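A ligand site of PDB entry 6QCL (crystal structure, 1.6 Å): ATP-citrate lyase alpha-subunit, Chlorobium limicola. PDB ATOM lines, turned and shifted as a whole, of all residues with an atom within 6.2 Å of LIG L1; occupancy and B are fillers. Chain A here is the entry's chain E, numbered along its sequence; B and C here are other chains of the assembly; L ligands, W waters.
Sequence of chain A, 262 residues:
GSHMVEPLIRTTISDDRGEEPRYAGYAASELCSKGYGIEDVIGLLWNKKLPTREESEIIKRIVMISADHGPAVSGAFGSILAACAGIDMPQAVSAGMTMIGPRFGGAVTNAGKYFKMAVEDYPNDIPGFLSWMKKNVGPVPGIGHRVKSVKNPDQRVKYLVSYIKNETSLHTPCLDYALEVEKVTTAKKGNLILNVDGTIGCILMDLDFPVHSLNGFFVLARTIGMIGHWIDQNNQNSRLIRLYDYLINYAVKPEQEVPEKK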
ATOM      1  N   SER A  66       6.142  34.474 -31.851  1.00  0.00           N
ATOM      2  CA  SER A  66       6.594  33.116 -31.590  1.00  0.00           C
ATOM      3  C   SER A  66       8.108  32.925 -31.691  1.00  0.00           C
ATOM      4  O   SER A  66       8.568  31.808 -31.455  1.00  0.00           O
ATOM      5  CB  SER A  66       5.940  32.182 -32.627  1.00  0.00           C
ATOM      6  OG  SER A  66       4.527  32.202 -32.522  1.00  0.00           O
ATOM      7  N   ASP A  68      10.853  33.514 -30.025  1.00  0.00           N
ATOM      8  CA  ASP A  68      11.679  32.982 -28.932  1.00  0.00           C
ATOM      9  C   ASP A  68      10.922  33.006 -27.620  1.00  0.00           C
ATOM     10  O   ASP A  68      10.116  33.903 -27.378  1.00  0.00           O
ATOM     11  CB  ASP A  68      13.007  33.769 -28.783  1.00  0.00           C
ATOM     12  CG  ASP A  68      14.015  32.944 -27.938  1.00  0.00           C
ATOM     13  OD1 ASP A  68      14.426  31.867 -28.387  1.00  0.00           O
ATOM     14  OD2 ASP A  68      14.247  33.317 -26.790  1.00  0.00           O
ATOM     15  N   HIS A  69      11.236  32.060 -26.739  1.00  0.00           N
ATOM     16  CA  HIS A  69      10.654  32.025 -25.416  1.00  0.00           C
ATOM     17  C   HIS A  69      11.679  31.562 -24.407  1.00  0.00           C
ATOM     18  O   HIS A  69      11.328  30.861 -23.457  1.00  0.00           O
ATOM     19  CB  HIS A  69       9.343  31.231 -25.337  1.00  0.00           C
ATOM     20  CG  HIS A  69       8.388  31.768 -24.303  1.00  0.00           C
ATOM     21  ND1 HIS A  69       7.686  30.928 -23.477  1.00  0.00           N
ATOM     22  CD2 HIS A  69       8.006  33.040 -24.044  1.00  0.00           C
ATOM     23  CE1 HIS A  69       6.909  31.701 -22.728  1.00  0.00           C
ATOM     24  NE2 HIS A  69       7.070  32.979 -23.025  1.00  0.00           N
ATOM     25  N   VAL A  73      13.389  26.181 -22.525  1.00  0.00           N
ATOM     26  CA  VAL A  73      12.510  25.328 -23.308  1.00  0.00           C
ATOM     27  C   VAL A  73      13.297  24.447 -24.273  1.00  0.00           C
ATOM     28  O   VAL A  73      14.424  24.765 -24.667  1.00  0.00           O
ATOM     29  CB  VAL A  73      11.395  26.134 -23.988  1.00  0.00           C
ATOM     30  CG1 VAL A  73      10.522  26.840 -22.948  1.00  0.00           C
ATOM     31  CG2 VAL A  73      11.935  27.136 -24.966  1.00  0.00           C
ATOM     32  N   PHE A 104       5.785  20.241 -27.389  1.00  0.00           N
ATOM     33  CA  PHE A 104       6.423  21.526 -27.518  1.00  0.00           C
ATOM     34  C   PHE A 104       6.346  22.033 -28.934  1.00  0.00           C
ATOM     35  O   PHE A 104       7.001  21.485 -29.795  1.00  0.00           O
ATOM     36  CB  PHE A 104       7.909  21.400 -27.076  1.00  0.00           C
ATOM     37  CG  PHE A 104       8.794  22.547 -27.469  1.00  0.00           C
ATOM     38  CD1 PHE A 104       8.522  23.832 -27.030  1.00  0.00           C
ATOM     39  CD2 PHE A 104       9.831  22.381 -28.370  1.00  0.00           C
ATOM     40  CE1 PHE A 104       9.259  24.916 -27.505  1.00  0.00           C
ATOM     41  CE2 PHE A 104      10.553  23.471 -28.851  1.00  0.00           C
ATOM     42  CZ  PHE A 104      10.272  24.726 -28.400  1.00  0.00           C
ATOM     43  N   GLY A 105       5.599  23.124 -29.145  1.00  0.00           N
ATOM     44  CA  GLY A 105       5.612  23.844 -30.385  1.00  0.00           C
ATOM     45  C   GLY A 105       4.894  23.291 -31.589  1.00  0.00           C
ATOM     46  O   GLY A 105       4.453  24.092 -32.409  1.00  0.00           O
ATOM     47  N   HIS A 145      -0.244  24.423 -20.833  1.00  0.00           N
ATOM     48  CA  HIS A 145       1.094  25.004 -20.846  1.00  0.00           C
ATOM     49  C   HIS A 145       1.818  24.623 -19.549  1.00  0.00           C
ATOM     50  O   HIS A 145       1.173  24.419 -18.530  1.00  0.00           O
ATOM     51  CB  HIS A 145       1.034  26.540 -20.971  1.00  0.00           C
ATOM     52  CG  HIS A 145       2.266  27.128 -21.553  1.00  0.00           C
ATOM     53  ND1 HIS A 145       3.295  27.606 -20.741  1.00  0.00           N
ATOM     54  CD2 HIS A 145       2.651  27.215 -22.848  1.00  0.00           C
ATOM     55  CE1 HIS A 145       4.256  27.995 -21.577  1.00  0.00           C
ATOM     56  NE2 HIS A 145       3.922  27.768 -22.844  1.00  0.00           N
ATOM     57  N   ARG A 146       3.152  24.525 -19.591  1.00  0.00           N
ATOM     58  CA  ARG A 146       3.915  24.214 -18.375  1.00  0.00           C
ATOM     59  C   ARG A 146       3.934  25.397 -17.385  1.00  0.00           C
ATOM     60  O   ARG A 146       3.933  25.158 -16.149  1.00  0.00           O
ATOM     61  CB  ARG A 146       5.352  23.808 -18.752  1.00  0.00           C
ATOM     62  CG  ARG A 146       6.284  23.587 -17.565  1.00  0.00           C
ATOM     63  CD  ARG A 146       5.789  22.550 -16.585  1.00  0.00           C
ATOM     64  NE  ARG A 146       5.670  21.233 -17.189  1.00  0.00           N
ATOM     65  CZ  ARG A 146       6.687  20.406 -17.450  1.00  0.00           C
ATOM     66  NH1 ARG A 146       6.467  19.223 -18.017  1.00  0.00           N
ATOM     67  NH2 ARG A 146       7.937  20.770 -17.179  1.00  0.00           N
ATOM     68  N   VAL A 147       4.016  26.657 -17.886  1.00  0.00           N
ATOM     69  CA  VAL A 147       4.163  27.826 -17.025  1.00  0.00           C
ATOM     70  C   VAL A 147       3.012  28.836 -17.088  1.00  0.00           C
ATOM     71  O   VAL A 147       2.712  29.438 -16.047  1.00  0.00           O
ATOM     72  CB  VAL A 147       5.533  28.509 -17.255  1.00  0.00           C
ATOM     73  CG1 VAL A 147       6.670  27.566 -16.855  1.00  0.00           C
ATOM     74  CG2 VAL A 147       5.754  28.963 -18.681  1.00  0.00           C
ATOM     75  N   LYS A 148       2.407  29.057 -18.257  1.00  0.00           N
ATOM     76  CA  LYS A 148       1.295  29.990 -18.419  1.00  0.00           C
ATOM     77  C   LYS A 148       0.006  29.327 -17.915  1.00  0.00           C
ATOM     78  O   LYS A 148      -0.160  28.112 -18.029  1.00  0.00           O
ATOM     79  CB  LYS A 148       1.148  30.405 -19.875  1.00  0.00           C
ATOM     80  CG  LYS A 148       2.376  31.101 -20.469  1.00  0.00           C
ATOM     81  CD  LYS A 148       2.718  32.409 -19.798  1.00  0.00           C
ATOM     82  CE  LYS A 148       3.719  33.193 -20.616  1.00  0.00           C
ATOM     83  NZ  LYS A 148       4.175  34.416 -19.892  1.00  0.00           N
ATOM     84  N   ASP A 154      -0.979  34.085 -20.697  1.00  0.00           N
ATOM     85  CA  ASP A 154      -0.029  34.229 -21.784  1.00  0.00           C
ATOM     86  C   ASP A 154      -0.436  35.465 -22.549  1.00  0.00           C
ATOM     87  O   ASP A 154      -1.347  35.398 -23.392  1.00  0.00           O
ATOM     88  CB  ASP A 154      -0.030  33.012 -22.691  1.00  0.00           C
ATOM     89  CG  ASP A 154       1.160  32.973 -23.633  1.00  0.00           C
ATOM     90  OD1 ASP A 154       1.786  34.027 -23.829  1.00  0.00           O
ATOM     91  OD2 ASP A 154       1.552  31.871 -24.034  1.00  0.00           O
ATOM     92  N   ARG A 156       0.985  36.662 -25.023  1.00  0.00           N
ATOM     93  CA  ARG A 156       1.121  36.466 -26.475  1.00  0.00           C
ATOM     94  C   ARG A 156      -0.228  36.065 -27.023  1.00  0.00           C
ATOM     95  O   ARG A 156      -0.605  36.541 -28.058  1.00  0.00           O
ATOM     96  CB  ARG A 156       2.139  35.381 -26.796  1.00  0.00           C
ATOM     97  CG  ARG A 156       3.589  35.702 -26.382  1.00  0.00           C
ATOM     98  CD  ARG A 156       4.509  34.505 -26.541  1.00  0.00           C
ATOM     99  NE  ARG A 156       4.096  33.382 -25.721  1.00  0.00           N
ATOM    100  CZ  ARG A 156       4.608  32.161 -25.799  1.00  0.00           C
ATOM    101  NH1 ARG A 156       5.618  31.907 -26.616  1.00  0.00           N
ATOM    102  NH2 ARG A 156       4.148  31.206 -25.010  1.00  0.00           N
ATOM    103  N   VAL A 196      -0.357  29.158 -27.329  1.00  0.00           N
ATOM    104  CA  VAL A 196       0.025  29.804 -28.579  1.00  0.00           C
ATOM    105  C   VAL A 196      -0.164  28.913 -29.776  1.00  0.00           C
ATOM    106  O   VAL A 196      -0.623  29.369 -30.816  1.00  0.00           O
ATOM    107  CB  VAL A 196       1.431  30.428 -28.561  1.00  0.00           C
ATOM    108  CG1 VAL A 196       1.451  31.622 -27.640  1.00  0.00           C
ATOM    109  CG2 VAL A 196       2.502  29.433 -28.187  1.00  0.00           C
ATOM    110  N   PHE A 218       5.350  27.970 -36.509  1.00  0.00           N
ATOM    111  CA  PHE A 218       6.136  27.857 -35.272  1.00  0.00           C
ATOM    112  C   PHE A 218       7.572  27.384 -35.602  1.00  0.00           C
ATOM    113  O   PHE A 218       8.536  27.923 -35.044  1.00  0.00           O
ATOM    114  CB  PHE A 218       5.490  26.875 -34.322  1.00  0.00           C
ATOM    115  CG  PHE A 218       6.181  26.884 -32.984  1.00  0.00           C
ATOM    116  CD1 PHE A 218       5.835  27.809 -32.009  1.00  0.00           C
ATOM    117  CD2 PHE A 218       7.240  26.024 -32.724  1.00  0.00           C
ATOM    118  CE1 PHE A 218       6.490  27.838 -30.774  1.00  0.00           C
ATOM    119  CE2 PHE A 218       7.940  26.091 -31.523  1.00  0.00           C
ATOM    120  CZ  PHE A 218       7.548  26.992 -30.553  1.00  0.00           C
ATOM    121  N   ARG A 222      10.480  29.869 -34.501  1.00  0.00           N
ATOM    122  CA  ARG A 222      11.395  29.477 -33.418  1.00  0.00           C
ATOM    123  C   ARG A 222      12.820  29.203 -33.891  1.00  0.00           C
ATOM    124  O   ARG A 222      13.757  29.294 -33.103  1.00  0.00           O
ATOM    125  CB  ARG A 222      10.792  28.300 -32.622  1.00  0.00           C
ATOM    126  CG  ARG A 222      11.455  28.016 -31.309  1.00  0.00           C
ATOM    127  CD  ARG A 222      11.595  29.222 -30.349  1.00  0.00           C
ATOM    128  NE  ARG A 222      10.307  29.893 -30.030  1.00  0.00           N
ATOM    129  CZ  ARG A 222       9.478  29.554 -29.043  1.00  0.00           C
ATOM    130  NH1 ARG A 222       8.350  30.202 -28.860  1.00  0.00           N
ATOM    131  NH2 ARG A 222       9.800  28.581 -28.195  1.00  0.00           N
ATOM    132  N   LEU B 240       7.553  16.496 -20.331  1.00  0.00           N
ATOM    133  CA  LEU B 240       8.407  17.494 -20.935  1.00  0.00           C
ATOM    134  C   LEU B 240       9.366  18.126 -19.947  1.00  0.00           C
ATOM    135  O   LEU B 240       8.987  18.407 -18.808  1.00  0.00           O
ATOM    136  CB  LEU B 240       7.495  18.575 -21.519  1.00  0.00           C
ATOM    137  CG  LEU B 240       8.096  19.674 -22.334  1.00  0.00           C
ATOM    138  CD1 LEU B 240       8.580  19.168 -23.689  1.00  0.00           C
ATOM    139  CD2 LEU B 240       7.027  20.727 -22.616  1.00  0.00           C
ATOM    140  N   ARG B 242      11.538  21.360 -18.814  1.00  0.00           N
ATOM    141  CA  ARG B 242      11.699  22.801 -18.927  1.00  0.00           C
ATOM    142  C   ARG B 242      12.645  23.179 -17.782  1.00  0.00           C
ATOM    143  O   ARG B 242      12.360  22.871 -16.626  1.00  0.00           O
ATOM    144  CB  ARG B 242      10.351  23.510 -18.867  1.00  0.00           C
ATOM    145  CG  ARG B 242      10.389  24.972 -19.335  1.00  0.00           C
ATOM    146  CD  ARG B 242       9.049  25.660 -19.074  1.00  0.00           C
ATOM    147  NE  ARG B 242       8.837  26.814 -19.948  1.00  0.00           N
ATOM    148  CZ  ARG B 242       9.351  28.023 -19.770  1.00  0.00           C
ATOM    149  NH1 ARG B 242      10.124  28.275 -18.731  1.00  0.00           N
ATOM    150  NH2 ARG B 242       9.105  28.995 -20.652  1.00  0.00           N
ATOM    151  N   ASP C  16      11.942  35.299 -20.912  1.00  0.00           N
ATOM    152  CA  ASP C  16      10.584  34.747 -21.035  1.00  0.00           C
ATOM    153  C   ASP C  16       9.812  34.776 -19.729  1.00  0.00           C
ATOM    154  O   ASP C  16       8.663  34.310 -19.705  1.00  0.00           O
ATOM    155  CB  ASP C  16      10.705  33.272 -21.466  1.00  0.00           C
ATOM    156  CG  ASP C  16      11.505  32.405 -20.504  1.00  0.00           C
ATOM    157  OD1 ASP C  16      12.693  32.757 -20.230  1.00  0.00           O
ATOM    158  OD2 ASP C  16      10.969  31.392 -20.042  1.00  0.00           O
HETATM  159  C1  LIG L   1       6.175  28.502 -25.839  1.00  0.00           C
HETATM  160  O1  LIG L   1       5.128  28.600 -25.223  1.00  0.00           O
HETATM  161  O2  LIG L   1       6.655  29.384 -26.669  1.00  0.00           O
HETATM  162  C2  LIG L   1       7.081  27.293 -25.726  1.00  0.00           C
HETATM  163  O3  LIG L   1       8.412  27.761 -25.758  1.00  0.00           O
HETATM  164  C3  LIG L   1       6.742  26.427 -24.523  1.00  0.00           C
HETATM  165  C4  LIG L   1       7.108  26.938 -23.139  1.00  0.00           C
HETATM  166  O4  LIG L   1       7.519  28.183 -23.091  1.00  0.00           O
HETATM  167  O5  LIG L   1       7.044  26.221 -22.140  1.00  0.00           O
HETATM  168  N1  LG2 L   2      -5.880  18.219 -22.746  1.00  0.00           N
HETATM  169  C1  LG2 L   2      -6.326  17.576 -21.667  1.00  0.00           C
HETATM  170  N2  LG2 L   2      -5.727  17.434 -20.473  1.00  0.00           N
HETATM  171  C2  LG2 L   2      -4.533  18.058 -20.453  1.00  0.00           C
HETATM  172  C3  LG2 L   2      -3.948  18.747 -21.505  1.00  0.00           C
HETATM  173  C4  LG2 L   2      -4.679  18.837 -22.698  1.00  0.00           C
HETATM  174  N3  LG2 L   2      -4.246  19.497 -23.764  1.00  0.00           N
HETATM  175  N4  LG2 L   2      -2.717  19.255 -21.123  1.00  0.00           N
HETATM  176  C5  LG2 L   2      -2.590  18.881 -19.871  1.00  0.00           C
HETATM  177  N5  LG2 L   2      -3.664  18.154 -19.402  1.00  0.00           N
HETATM  178  C6  LG2 L   2      -3.831  17.617 -18.054  1.00  0.00           C
HETATM  179  C7  LG2 L   2      -3.093  16.300 -17.856  1.00  0.00           C
HETATM  180  O1  LG2 L   2      -3.985  15.234 -18.153  1.00  0.00           O
HETATM  181  C8  LG2 L   2      -2.717  16.399 -16.388  1.00  0.00           C
HETATM  182  O2  LG2 L   2      -3.899  16.147 -15.592  1.00  0.00           O
HETATM  183  P1  LG2 L   2      -3.816  15.299 -14.196  1.00  0.00           P
HETATM  184  O3  LG2 L   2      -3.065  16.114 -13.188  1.00  0.00           O
HETATM  185  O4  LG2 L   2      -5.251  14.960 -13.823  1.00  0.00           O
HETATM  186  O5  LG2 L   2      -3.112  13.992 -14.571  1.00  0.00           O
HETATM  187  C9  LG2 L   2      -2.386  17.879 -16.227  1.00  0.00           C
HETATM  188  O6  LG2 L   2      -3.284  18.543 -17.143  1.00  0.00           O
HETATM  189  C10 LG2 L   2      -0.973  18.286 -16.525  1.00  0.00           C
HETATM  190  O7  LG2 L   2      -0.552  17.582 -17.702  1.00  0.00           O
HETATM  191  P2  LG2 L   2       0.964  17.102 -17.991  1.00  0.00           P
HETATM  192  O8  LG2 L   2       1.023  16.707 -19.418  1.00  0.00           O
HETATM  193  O9  LG2 L   2       1.372  16.129 -16.890  1.00  0.00           O
HETATM  194  O10 LG2 L   2       1.677  18.483 -17.716  1.00  0.00           O
HETATM  195  P3  LG2 L   2       2.664  19.387 -18.562  1.00  0.00           P
HETATM  196  O11 LG2 L   2       3.038  20.590 -17.843  1.00  0.00           O
HETATM  197  O12 LG2 L   2       3.832  18.508 -18.946  1.00  0.00           O
HETATM  198  O13 LG2 L   2       1.737  19.782 -19.814  1.00  0.00           O
HETATM  199  C11 LG2 L   2       1.827  20.340 -22.167  1.00  0.00           C
HETATM  200  C12 LG2 L   2       2.215  20.757 -20.751  1.00  0.00           C
HETATM  201  C13 LG2 L   2       2.853  19.295 -22.657  1.00  0.00           C
HETATM  202  C14 LG2 L   2       1.890  21.596 -23.049  1.00  0.00           C
HETATM  203  C15 LG2 L   2       0.404  19.735 -22.229  1.00  0.00           C
HETATM  204  O14 LG2 L   2      -0.515  20.704 -21.732  1.00  0.00           O
HETATM  205  C16 LG2 L   2      -0.017  19.208 -23.599  1.00  0.00           C
HETATM  206  O15 LG2 L   2       0.422  18.124 -24.008  1.00  0.00           O
HETATM  207  N6  LG2 L   2      -0.837  19.980 -24.314  1.00  0.00           N
HETATM  208  C17 LG2 L   2      -1.313  19.633 -25.644  1.00  0.00           C
HETATM  209  C18 LG2 L   2      -0.249  19.837 -26.708  1.00  0.00           C
HETATM  210  C19 LG2 L   2       0.045  21.298 -26.949  1.00  0.00           C
HETATM  211  O16 LG2 L   2      -0.885  22.073 -27.186  1.00  0.00           O
HETATM  212  N7  LG2 L   2       1.329  21.666 -26.887  1.00  0.00           N
HETATM  213  C20 LG2 L   2       1.787  23.034 -27.158  1.00  0.00           C
HETATM  214  C21 LG2 L   2       2.043  23.875 -25.909  1.00  0.00           C
HETATM  215  S1  LG2 L   2       2.260  25.628 -26.420  1.00  0.00           S
HETATM  216  C22 LG2 L   2       3.867  25.496 -27.119  1.00  0.00           C
HETATM  217  O17 LG2 L   2       4.602  24.587 -26.861  1.00  0.00           O
HETATM  218  C23 LG2 L   2       4.306  26.747 -27.813  1.00  0.00           C
HETATM  219  O   HOH W   1       8.127  23.775 -23.027  1.00  0.00           O
HETATM  220  O   HOH W   2       4.711  24.528 -22.111  1.00  0.00           O
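Merely in contact with LIG L1: Val 73 and Phe 104.
Hydrophobic or aromatic side chains that line LIG L1: His 69, Val 73, Phe 104 and His 145.
Water W2 lies within hydrogen-bond range of an oxygen (O5) of LIG L1 (2.9 Å), the backbone NH (N) of Arg 146 (3.0 Å) and a ring nitrogen (NE2) of His 145 (3.4 Å).
An oxygen (O1) of LIG L1 lies within hydrogen-bond range of a ring nitrogen (NE2) of His 145.
The guanidinium group of Arg 156 lies within salt-bridge range of an oxygen (O2) of LIG L1, 2.7 Å away.
A ring nitrogen (ND1) of His 69 lies within hydrogen-bond range of an oxygen (O4) of LIG L1 (2.8 Å).
The guanidinium group of Arg 242 of chain B lies within salt-bridge range of an oxygen (O5) of LIG L1, 2.9 Å away.
The backbone NH (N) of Gly 105 is in hydrogen-bond range of an oxygen (O17) of LG2 L2, 2.9 Å away.
The guanidinium group of Arg 222 is in salt-bridge range of an oxygen (O2) of LIG L1, 2.9 Å away.
The guanidinium group (NE) of Arg 146 lies within salt-bridge range of an oxygen (O11) of LG2 L2 (2.8 Å).
A ring nitrogen (ND1) of His 145 sits at hydrogen-bond distance from the backbone NH (N) of Lys 148, 3.0 Å away.
The guanidinium group (NE) of Arg 222 is in hydrogen-bond range of the backbone carbonyl oxygen (O) of Ser 66 (3.0 Å).
OD2 of Asp 16 of chain C lies within salt-bridge range of NH2 of Arg 242 of chain B.
OD2 of Asp 154 lies within salt-bridge range of NH2 of Arg 156 (2.9 Å).
ND1 of His 145 lies within hydrogen-bond range of N of Val 147, at 3.1 Å.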
